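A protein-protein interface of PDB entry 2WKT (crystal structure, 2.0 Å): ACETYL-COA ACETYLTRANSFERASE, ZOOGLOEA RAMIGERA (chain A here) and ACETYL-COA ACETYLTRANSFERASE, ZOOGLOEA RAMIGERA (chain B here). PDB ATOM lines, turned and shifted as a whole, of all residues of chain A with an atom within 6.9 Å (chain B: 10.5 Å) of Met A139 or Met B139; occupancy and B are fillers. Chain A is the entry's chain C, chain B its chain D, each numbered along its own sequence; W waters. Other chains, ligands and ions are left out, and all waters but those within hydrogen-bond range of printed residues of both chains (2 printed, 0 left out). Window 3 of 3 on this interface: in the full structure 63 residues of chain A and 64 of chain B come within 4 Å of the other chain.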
ATOM      1  N   PRO A 123      26.973 -12.463  10.218  1.00  0.00           N
ATOM      2  CA  PRO A 123      26.883 -12.315   8.759  1.00  0.00           C
ATOM      3  C   PRO A 123      28.206 -12.378   8.005  1.00  0.00           C
ATOM      4  O   PRO A 123      29.311 -12.372   8.546  1.00  0.00           O
ATOM      5  CB  PRO A 123      26.309 -10.903   8.578  1.00  0.00           C
ATOM      6  CG  PRO A 123      26.465 -10.215   9.927  1.00  0.00           C
ATOM      7  CD  PRO A 123      27.105 -11.164  10.891  1.00  0.00           C
ATOM      8  N   HIS A 124      28.055 -12.422   6.696  1.00  0.00           N
ATOM      9  CA  HIS A 124      29.155 -12.249   5.804  1.00  0.00           C
ATOM     10  C   HIS A 124      29.242 -10.747   5.493  1.00  0.00           C
ATOM     11  O   HIS A 124      28.227 -10.060   5.450  1.00  0.00           O
ATOM     12  CB  HIS A 124      28.899 -13.078   4.551  1.00  0.00           C
ATOM     13  CG  HIS A 124      29.202 -14.531   4.719  1.00  0.00           C
ATOM     14  ND1 HIS A 124      28.385 -15.383   5.429  1.00  0.00           N
ATOM     15  CD2 HIS A 124      30.225 -15.287   4.259  1.00  0.00           C
ATOM     16  CE1 HIS A 124      28.891 -16.602   5.399  1.00  0.00           C
ATOM     17  NE2 HIS A 124      30.006 -16.573   4.690  1.00  0.00           N
ATOM     18  N   CYS A 125      30.450 -10.238   5.286  1.00  0.00           N
ATOM     19  CA  CYS A 125      30.626  -8.812   5.009  1.00  0.00           C
ATOM     20  C   CYS A 125      31.683  -8.543   3.941  1.00  0.00           C
ATOM     21  O   CYS A 125      32.494  -9.416   3.612  1.00  0.00           O
ATOM     22  CB  CYS A 125      31.010  -8.068   6.299  1.00  0.00           C
ATOM     23  SG  CYS A 125      32.656  -8.472   6.969  1.00  0.00           S
ATOM     24  N   ALA A 126      31.672  -7.316   3.423  1.00  0.00           N
ATOM     25  CA  ALA A 126      32.661  -6.829   2.462  1.00  0.00           C
ATOM     26  C   ALA A 126      32.746  -5.321   2.582  1.00  0.00           C
ATOM     27  O   ALA A 126      31.718  -4.638   2.682  1.00  0.00           O
ATOM     28  CB  ALA A 126      32.266  -7.222   1.014  1.00  0.00           C
ATOM     29  N   LEU A 128      32.986  -2.069   0.818  1.00  0.00           N
ATOM     30  CA  LEU A 128      32.542  -1.793  -0.543  1.00  0.00           C
ATOM     31  C   LEU A 128      32.370  -0.314  -0.839  1.00  0.00           C
ATOM     32  O   LEU A 128      31.768   0.060  -1.854  1.00  0.00           O
ATOM     33  CB  LEU A 128      31.213  -2.515  -0.828  1.00  0.00           C
ATOM     34  CG  LEU A 128      31.288  -4.029  -1.020  1.00  0.00           C
ATOM     35  CD1 LEU A 128      29.889  -4.656  -1.055  1.00  0.00           C
ATOM     36  CD2 LEU A 128      32.063  -4.339  -2.285  1.00  0.00           C
ATOM     37  N   PHE A 137      35.245 -10.411  -5.645  1.00  0.00           N
ATOM     38  CA  PHE A 137      35.719 -10.051  -4.306  1.00  0.00           C
ATOM     39  C   PHE A 137      35.158 -11.009  -3.261  1.00  0.00           C
ATOM     40  O   PHE A 137      34.175 -11.719  -3.503  1.00  0.00           O
ATOM     41  CB  PHE A 137      35.401  -8.598  -3.938  1.00  0.00           C
ATOM     42  CG  PHE A 137      33.925  -8.282  -3.827  1.00  0.00           C
ATOM     43  CD1 PHE A 137      33.207  -7.844  -4.931  1.00  0.00           C
ATOM     44  CD2 PHE A 137      33.277  -8.363  -2.612  1.00  0.00           C
ATOM     45  CE1 PHE A 137      31.852  -7.533  -4.820  1.00  0.00           C
ATOM     46  CE2 PHE A 137      31.936  -8.047  -2.486  1.00  0.00           C
ATOM     47  CZ  PHE A 137      31.215  -7.637  -3.585  1.00  0.00           C
ATOM     48  N   LYS A 138      35.789 -11.017  -2.096  1.00  0.00           N
ATOM     49  CA  LYS A 138      35.375 -11.921  -1.034  1.00  0.00           C
ATOM     50  C   LYS A 138      34.279 -11.335  -0.168  1.00  0.00           C
ATOM     51  O   LYS A 138      34.363 -10.186   0.261  1.00  0.00           O
ATOM     52  CB  LYS A 138      36.561 -12.294  -0.139  1.00  0.00           C
ATOM     53  CG  LYS A 138      37.508 -13.308  -0.746  1.00  0.00           C
ATOM     54  CD  LYS A 138      38.560 -13.728   0.276  1.00  0.00           C
ATOM     55  CE  LYS A 138      39.774 -14.364  -0.394  1.00  0.00           C
ATOM     56  NZ  LYS A 138      39.400 -15.508  -1.275  1.00  0.00           N
ATOM     57  N   MET A 139      33.255 -12.146   0.083  1.00  0.00           N
ATOM     58  CA  MET A 139      32.300 -11.896   1.158  1.00  0.00           C
ATOM     59  C   MET A 139      32.786 -12.692   2.358  1.00  0.00           C
ATOM     60  O   MET A 139      32.784 -13.917   2.340  1.00  0.00           O
ATOM     61  CB  MET A 139      30.885 -12.338   0.747  1.00  0.00           C
ATOM     62  CG  MET A 139      30.170 -11.324  -0.158  1.00  0.00           C
ATOM     63  SD  MET A 139      29.633  -9.868   0.767  1.00  0.00           S
ATOM     64  CE  MET A 139      28.200 -10.566   1.596  1.00  0.00           C
ATOM     65  N   ILE A 140      33.217 -11.990   3.398  1.00  0.00           N
ATOM     66  CA  ILE A 140      33.913 -12.631   4.515  1.00  0.00           C
ATOM     67  C   ILE A 140      32.953 -13.110   5.600  1.00  0.00           C
ATOM     68  O   ILE A 140      32.097 -12.358   6.044  1.00  0.00           O
ATOM     69  CB  ILE A 140      34.931 -11.659   5.149  1.00  0.00           C
ATOM     70  CG1 ILE A 140      35.982 -11.221   4.119  1.00  0.00           C
ATOM     71  CG2 ILE A 140      35.581 -12.277   6.400  1.00  0.00           C
ATOM     72  CD1 ILE A 140      36.791 -12.354   3.520  1.00  0.00           C
ATOM     73  N   ASP A 141      33.093 -14.371   6.006  1.00  0.00           N
ATOM     74  CA  ASP A 141      32.337 -14.914   7.118  1.00  0.00           C
ATOM     75  C   ASP A 141      32.897 -14.343   8.417  1.00  0.00           C
ATOM     76  O   ASP A 141      33.974 -14.751   8.868  1.00  0.00           O
ATOM     77  CB  ASP A 141      32.481 -16.426   7.127  1.00  0.00           C
ATOM     78  CG  ASP A 141      31.581 -17.094   8.147  1.00  0.00           C
ATOM     79  OD1 ASP A 141      31.145 -16.417   9.117  1.00  0.00           O
ATOM     80  OD2 ASP A 141      31.321 -18.307   7.972  1.00  0.00           O
ATOM     81  N   THR A 142      32.204 -13.377   9.009  1.00  0.00           N
ATOM     82  CA  THR A 142      32.719 -12.778  10.252  1.00  0.00           C
ATOM     83  C   THR A 142      32.954 -13.797  11.367  1.00  0.00           C
ATOM     84  O   THR A 142      33.831 -13.603  12.210  1.00  0.00           O
ATOM     85  CB  THR A 142      31.805 -11.658  10.806  1.00  0.00           C
ATOM     86  OG1 THR A 142      30.486 -12.171  11.045  1.00  0.00           O
ATOM     87  CG2 THR A 142      31.739 -10.503   9.835  1.00  0.00           C
ATOM     88  N   GLY B  61      34.970  -7.604  10.407  1.00  0.00           N
ATOM     89  CA  GLY B  61      35.913  -7.896   9.347  1.00  0.00           C
ATOM     90  C   GLY B  61      37.391  -7.695   9.649  1.00  0.00           C
ATOM     91  O   GLY B  61      38.238  -7.970   8.802  1.00  0.00           O
ATOM     92  N   ALA B 122      34.424   0.256   7.754  1.00  0.00           N
ATOM     93  CA  ALA B 122      33.270  -0.553   8.155  1.00  0.00           C
ATOM     94  C   ALA B 122      32.583  -1.125   6.915  1.00  0.00           C
ATOM     95  O   ALA B 122      32.239  -0.396   5.985  1.00  0.00           O
ATOM     96  CB  ALA B 122      32.292   0.259   9.003  1.00  0.00           C
ATOM     97  N   PRO B 123      32.399  -2.446   6.893  1.00  0.00           N
ATOM     98  CA  PRO B 123      31.873  -3.110   5.702  1.00  0.00           C
ATOM     99  C   PRO B 123      30.359  -3.199   5.691  1.00  0.00           C
ATOM    100  O   PRO B 123      29.686  -2.904   6.690  1.00  0.00           O
ATOM    101  CB  PRO B 123      32.450  -4.516   5.822  1.00  0.00           C
ATOM    102  CG  PRO B 123      32.529  -4.751   7.297  1.00  0.00           C
ATOM    103  CD  PRO B 123      32.754  -3.403   7.955  1.00  0.00           C
ATOM    104  N   HIS B 124      29.841  -3.615   4.541  1.00  0.00           N
ATOM    105  CA  HIS B 124      28.445  -4.003   4.382  1.00  0.00           C
ATOM    106  C   HIS B 124      28.314  -5.488   4.710  1.00  0.00           C
ATOM    107  O   HIS B 124      29.290  -6.235   4.607  1.00  0.00           O
ATOM    108  CB  HIS B 124      28.009  -3.748   2.940  1.00  0.00           C
ATOM    109  CG  HIS B 124      27.684  -2.318   2.654  1.00  0.00           C
ATOM    110  ND1 HIS B 124      28.651  -1.341   2.546  1.00  0.00           N
ATOM    111  CD2 HIS B 124      26.498  -1.700   2.450  1.00  0.00           C
ATOM    112  CE1 HIS B 124      28.073  -0.180   2.291  1.00  0.00           C
ATOM    113  NE2 HIS B 124      26.767  -0.371   2.222  1.00  0.00           N
ATOM    114  N   CYS B 125      27.125  -5.925   5.119  1.00  0.00           N
ATOM    115  CA  CYS B 125      26.972  -7.300   5.585  1.00  0.00           C
ATOM    116  C   CYS B 125      25.558  -7.821   5.402  1.00  0.00           C
ATOM    117  O   CYS B 125      24.613  -7.062   5.281  1.00  0.00           O
ATOM    118  CB  CYS B 125      27.350  -7.407   7.073  1.00  0.00           C
ATOM    119  SG  CYS B 125      26.133  -6.680   8.213  1.00  0.00           S
ATOM    120  N   ALA B 126      25.419  -9.136   5.417  1.00  0.00           N
ATOM    121  CA  ALA B 126      24.106  -9.736   5.443  1.00  0.00           C
ATOM    122  C   ALA B 126      24.245 -11.092   6.066  1.00  0.00           C
ATOM    123  O   ALA B 126      25.293 -11.734   5.925  1.00  0.00           O
ATOM    124  CB  ALA B 126      23.538  -9.862   4.019  1.00  0.00           C
ATOM    125  N   HIS B 127      23.184 -11.540   6.733  1.00  0.00           N
ATOM    126  CA  HIS B 127      23.155 -12.877   7.288  1.00  0.00           C
ATOM    127  C   HIS B 127      22.642 -13.826   6.214  1.00  0.00           C
ATOM    128  O   HIS B 127      21.492 -13.730   5.795  1.00  0.00           O
ATOM    129  CB  HIS B 127      22.286 -12.926   8.554  1.00  0.00           C
ATOM    130  CG  HIS B 127      22.012 -14.315   9.042  1.00  0.00           C
ATOM    131  ND1 HIS B 127      20.735 -14.798   9.229  1.00  0.00           N
ATOM    132  CD2 HIS B 127      22.850 -15.320   9.387  1.00  0.00           C
ATOM    133  CE1 HIS B 127      20.797 -16.045   9.661  1.00  0.00           C
ATOM    134  NE2 HIS B 127      22.069 -16.388   9.759  1.00  0.00           N
ATOM    135  N   LEU B 128      23.507 -14.748   5.792  1.00  0.00           N
ATOM    136  CA  LEU B 128      23.262 -15.587   4.633  1.00  0.00           C
ATOM    137  C   LEU B 128      23.379 -17.075   4.931  1.00  0.00           C
ATOM    138  O   LEU B 128      23.380 -17.888   4.022  1.00  0.00           O
ATOM    139  CB  LEU B 128      24.264 -15.214   3.540  1.00  0.00           C
ATOM    140  CG  LEU B 128      24.144 -13.775   3.036  1.00  0.00           C
ATOM    141  CD1 LEU B 128      25.350 -13.414   2.184  1.00  0.00           C
ATOM    142  CD2 LEU B 128      22.847 -13.590   2.250  1.00  0.00           C
ATOM    143  N   ARG B 129      23.484 -17.443   6.204  1.00  0.00           N
ATOM    144  CA  ARG B 129      23.706 -18.848   6.550  1.00  0.00           C
ATOM    145  C   ARG B 129      22.535 -19.751   6.179  1.00  0.00           C
ATOM    146  O   ARG B 129      22.723 -20.907   5.795  1.00  0.00           O
ATOM    147  CB  ARG B 129      24.049 -18.996   8.054  1.00  0.00           C
ATOM    148  CG  ARG B 129      25.522 -18.889   8.322  1.00  0.00           C
ATOM    149  CD  ARG B 129      25.879 -19.099   9.807  1.00  0.00           C
ATOM    150  NE  ARG B 129      26.815 -18.070  10.215  1.00  0.00           N
ATOM    151  CZ  ARG B 129      28.039 -17.931   9.713  1.00  0.00           C
ATOM    152  NH1 ARG B 129      28.485 -18.780   8.791  1.00  0.00           N
ATOM    153  NH2 ARG B 129      28.819 -16.949  10.139  1.00  0.00           N
ATOM    154  N   VAL B 132      18.917 -17.309   0.970  1.00  0.00           N
ATOM    155  CA  VAL B 132      17.784 -16.511   0.557  1.00  0.00           C
ATOM    156  C   VAL B 132      17.082 -17.297  -0.529  1.00  0.00           C
ATOM    157  O   VAL B 132      17.574 -17.387  -1.656  1.00  0.00           O
ATOM    158  CB  VAL B 132      18.243 -15.167  -0.001  1.00  0.00           C
ATOM    159  CG1 VAL B 132      17.040 -14.260  -0.247  1.00  0.00           C
ATOM    160  CG2 VAL B 132      19.225 -14.523   0.954  1.00  0.00           C
ATOM    161  N   GLY B 135      13.779 -13.770  -3.868  1.00  0.00           N
ATOM    162  CA  GLY B 135      13.527 -12.362  -3.612  1.00  0.00           C
ATOM    163  C   GLY B 135      14.751 -11.562  -3.214  1.00  0.00           C
ATOM    164  O   GLY B 135      15.738 -12.095  -2.713  1.00  0.00           O
ATOM    165  N   ASP B 136      14.676 -10.259  -3.422  1.00  0.00           N
ATOM    166  CA  ASP B 136      15.761  -9.366  -3.057  1.00  0.00           C
ATOM    167  C   ASP B 136      16.024  -9.387  -1.542  1.00  0.00           C
ATOM    168  O   ASP B 136      15.129  -9.714  -0.773  1.00  0.00           O
ATOM    169  CB  ASP B 136      15.417  -7.945  -3.519  1.00  0.00           C
ATOM    170  CG  ASP B 136      15.124  -7.869  -5.021  1.00  0.00           C
ATOM    171  OD1 ASP B 136      15.352  -8.873  -5.740  1.00  0.00           O
ATOM    172  OD2 ASP B 136      14.654  -6.807  -5.486  1.00  0.00           O
ATOM    173  N   PHE B 137      17.265  -9.102  -1.140  1.00  0.00           N
ATOM    174  CA  PHE B 137      17.602  -8.825   0.265  1.00  0.00           C
ATOM    175  C   PHE B 137      18.538  -7.631   0.349  1.00  0.00           C
ATOM    176  O   PHE B 137      19.022  -7.127  -0.670  1.00  0.00           O
ATOM    177  CB  PHE B 137      18.222 -10.032   0.984  1.00  0.00           C
ATOM    178  CG  PHE B 137      19.578 -10.457   0.457  1.00  0.00           C
ATOM    179  CD1 PHE B 137      20.739 -10.030   1.074  1.00  0.00           C
ATOM    180  CD2 PHE B 137      19.684 -11.321  -0.634  1.00  0.00           C
ATOM    181  CE1 PHE B 137      21.991 -10.430   0.614  1.00  0.00           C
ATOM    182  CE2 PHE B 137      20.934 -11.732  -1.110  1.00  0.00           C
ATOM    183  CZ  PHE B 137      22.090 -11.287  -0.485  1.00  0.00           C
ATOM    184  N   LYS B 138      18.798  -7.181   1.566  1.00  0.00           N
ATOM    185  CA  LYS B 138      19.596  -5.985   1.765  1.00  0.00           C
ATOM    186  C   LYS B 138      21.012  -6.277   2.241  1.00  0.00           C
ATOM    187  O   LYS B 138      21.230  -7.088   3.136  1.00  0.00           O
ATOM    188  CB  LYS B 138      18.908  -5.054   2.761  1.00  0.00           C
ATOM    189  CG  LYS B 138      17.701  -4.318   2.195  1.00  0.00           C
ATOM    190  CD  LYS B 138      17.110  -3.360   3.210  1.00  0.00           C
ATOM    191  CE  LYS B 138      16.237  -2.315   2.524  1.00  0.00           C
ATOM    192  NZ  LYS B 138      15.723  -1.293   3.483  1.00  0.00           N
ATOM    193  N   MET B 139      21.974  -5.605   1.629  1.00  0.00           N
ATOM    194  CA  MET B 139      23.300  -5.511   2.201  1.00  0.00           C
ATOM    195  C   MET B 139      23.316  -4.288   3.103  1.00  0.00           C
ATOM    196  O   MET B 139      23.031  -3.171   2.670  1.00  0.00           O
ATOM    197  CB  MET B 139      24.355  -5.434   1.115  1.00  0.00           C
ATOM    198  CG  MET B 139      24.555  -6.762   0.426  1.00  0.00           C
ATOM    199  SD  MET B 139      25.634  -7.824   1.394  1.00  0.00           S
ATOM    200  CE  MET B 139      27.216  -7.047   1.051  1.00  0.00           C
ATOM    201  N   ILE B 140      23.617  -4.533   4.372  1.00  0.00           N
ATOM    202  CA  ILE B 140      23.453  -3.537   5.423  1.00  0.00           C
ATOM    203  C   ILE B 140      24.773  -2.879   5.750  1.00  0.00           C
ATOM    204  O   ILE B 140      25.783  -3.549   5.984  1.00  0.00           O
ATOM    205  CB  ILE B 140      22.867  -4.173   6.714  1.00  0.00           C
ATOM    206  CG1 ILE B 140      21.457  -4.691   6.463  1.00  0.00           C
ATOM    207  CG2 ILE B 140      22.844  -3.179   7.860  1.00  0.00           C
ATOM    208  CD1 ILE B 140      21.415  -6.152   6.124  1.00  0.00           C
ATOM    209  N   ASP B 141      24.771  -1.555   5.759  1.00  0.00           N
ATOM    210  CA  ASP B 141      25.970  -0.819   6.097  1.00  0.00           C
ATOM    211  C   ASP B 141      26.176  -0.907   7.614  1.00  0.00           C
ATOM    212  O   ASP B 141      25.391  -0.341   8.373  1.00  0.00           O
ATOM    213  CB  ASP B 141      25.815   0.629   5.638  1.00  0.00           C
ATOM    214  CG  ASP B 141      27.043   1.465   5.928  1.00  0.00           C
ATOM    215  OD1 ASP B 141      27.830   1.058   6.809  1.00  0.00           O
ATOM    216  OD2 ASP B 141      27.217   2.521   5.279  1.00  0.00           O
ATOM    217  N   THR B 142      27.206  -1.625   8.058  1.00  0.00           N
ATOM    218  CA  THR B 142      27.410  -1.798   9.500  1.00  0.00           C
ATOM    219  C   THR B 142      27.642  -0.489  10.233  1.00  0.00           C
ATOM    220  O   THR B 142      27.334  -0.374  11.428  1.00  0.00           O
ATOM    221  CB  THR B 142      28.582  -2.756   9.851  1.00  0.00           C
ATOM    222  OG1 THR B 142      29.804  -2.271   9.272  1.00  0.00           O
ATOM    223  CG2 THR B 142      28.294  -4.180   9.385  1.00  0.00           C
ATOM    224  N   MET B 143      28.245   0.483   9.557  1.00  0.00           N
ATOM    225  CA  MET B 143      28.453   1.794  10.165  1.00  0.00           C
ATOM    226  C   MET B 143      27.106   2.375  10.574  1.00  0.00           C
ATOM    227  O   MET B 143      26.933   2.862  11.702  1.00  0.00           O
ATOM    228  CB  MET B 143      29.161   2.739   9.200  1.00  0.00           C
ATOM    229  CG  MET B 143      29.333   4.148   9.718  1.00  0.00           C
ATOM    230  SD  MET B 143      30.068   5.250   8.491  1.00  0.00           S
ATOM    231  CE  MET B 143      28.701   5.439   7.353  1.00  0.00           C
ATOM    232  N   ILE B 144      26.149   2.312   9.654  1.00  0.00           N
ATOM    233  CA  ILE B 144      24.833   2.866   9.919  1.00  0.00           C
ATOM    234  C   ILE B 144      24.014   1.997  10.885  1.00  0.00           C
ATOM    235  O   ILE B 144      23.470   2.490  11.870  1.00  0.00           O
ATOM    236  CB  ILE B 144      24.062   3.104   8.620  1.00  0.00           C
ATOM    237  CG1 ILE B 144      24.811   4.121   7.764  1.00  0.00           C
ATOM    238  CG2 ILE B 144      22.652   3.601   8.917  1.00  0.00           C
ATOM    239  CD1 ILE B 144      24.343   4.146   6.345  1.00  0.00           C
ATOM    240  N   LYS B 145      23.946   0.703  10.610  1.00  0.00           N
ATOM    241  CA  LYS B 145      23.144  -0.201  11.420  1.00  0.00           C
ATOM    242  C   LYS B 145      23.635  -0.294  12.858  1.00  0.00           C
ATOM    243  O   LYS B 145      22.872  -0.077  13.791  1.00  0.00           O
ATOM    244  CB  LYS B 145      23.149  -1.600  10.817  1.00  0.00           C
ATOM    245  CG  LYS B 145      22.265  -2.588  11.557  1.00  0.00           C
ATOM    246  CD  LYS B 145      20.811  -2.188  11.428  1.00  0.00           C
ATOM    247  CE  LYS B 145      19.885  -3.298  11.900  1.00  0.00           C
ATOM    248  NZ  LYS B 145      18.448  -2.939  11.675  1.00  0.00           N
ATOM    249  N   ASP B 146      24.904  -0.655  13.019  1.00  0.00           N
ATOM    250  CA  ASP B 146      25.477  -0.922  14.341  1.00  0.00           C
ATOM    251  C   ASP B 146      26.045   0.338  14.988  1.00  0.00           C
ATOM    252  O   ASP B 146      26.299   0.379  16.202  1.00  0.00           O
ATOM    253  CB  ASP B 146      26.560  -2.007  14.239  1.00  0.00           C
ATOM    254  CG  ASP B 146      26.075  -3.264  13.503  1.00  0.00           C
ATOM    255  OD1 ASP B 146      24.867  -3.559  13.548  1.00  0.00           O
ATOM    256  OD2 ASP B 146      26.905  -3.977  12.902  1.00  0.00           O
HETATM  257  O   HOH W   1      31.604  -1.031   3.331  1.00  0.00           O
HETATM  258  O   HOH W   2      25.991 -15.136   7.508  1.00  0.00           O
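N of His B124 lies within hydrogen-bond range of O of Ala A126.
NH2 of Arg B129 lies within salt-bridge range of OD1 of Asp A141, 2.6 Å away.
The backbone carbonyl oxygen (O) of Ala B126 lies within hydrogen-bond range of the backbone NH (N) of His A124 (2.9 Å).
The backbone carbonyl oxygen of Cys A125 is in hydrogen-bond range of the backbone NH of Ile A140, 2.7 Å away.
The backbone NH (N) of Cys B125 lies within hydrogen-bond range of the backbone carbonyl oxygen (O) of Ile B140.
O of Pro A123 is in hydrogen-bond range of OG1 of Thr A142, at 2.8 Å.
The side-chain hydroxyl (OG1) of Thr B142 sits at hydrogen-bond distance from the backbone carbonyl oxygen (O) of Pro B123 (2.7 Å).
Pro A123 touches Cys B125 (CG to SG, 3.9 Å).
Pro A123 touches Ala B126.
Pro A123 touches His B127 (CB to N, 3.7 Å).
CA of Cys B125 touches O of His A124, at 3.0 Å.
Cys A125 touches Pro B123.
His B124 touches Cys A125.
Cys B125 touches Cys A125.
Ala A126 touches Pro B123 (O to CB, 3.2 Å).
CE of Met A139 touches CE of Met B139, 3.7 Å away.
Of the printed residues of chain B, Pro A123 touches Cys B125 (3.9 Å), Ala B126 (3.0 Å) and His B127 (3.7 Å).
His A124 touches two residues of chain B.
Cys A125 touches just these residues of chain B: Pro B123 (3.7 Å), His B124 (2.9 Å) and Cys B125 (3.8 Å).
Ala A126 touches two residues of chain B.
Met A139 touches one residue of chain B.
No residue of chain B comes within 4 Å of Ile A140.
Printed residues of chain B within 4 Å of Asp A141: Arg B129.
Gly B61 touches none of the printed residues of chain A.
Of the printed residues of chain A, Pro B123 touches Cys A125 (3.7 Å) and Ala A126 (3.2 Å).
Met B139 touches one residue of chain A.
Ile B140 touches none of the printed residues of chain A.
The nearest printed residue of chain B that does not touch Asp A141 is Gly B61 (7.1 Å).
Hydrophobic or aromatic side chains of chain B that line the printed part of chain A: Pro B123, His B124 and Met B139.
Among the printed residues, 12 pairs touch across the chains.
Water W1 lies within hydrogen-bond range of O of Ala B122 (2.8 Å), N of Leu A128 (3.1 Å) and ND1 of His B124 (3.1 Å).
Water W2 bridges the backbone NH (N) of Leu B128 (3.0 Å) and a ring nitrogen (ND1) of His A124 (3.2 Å).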
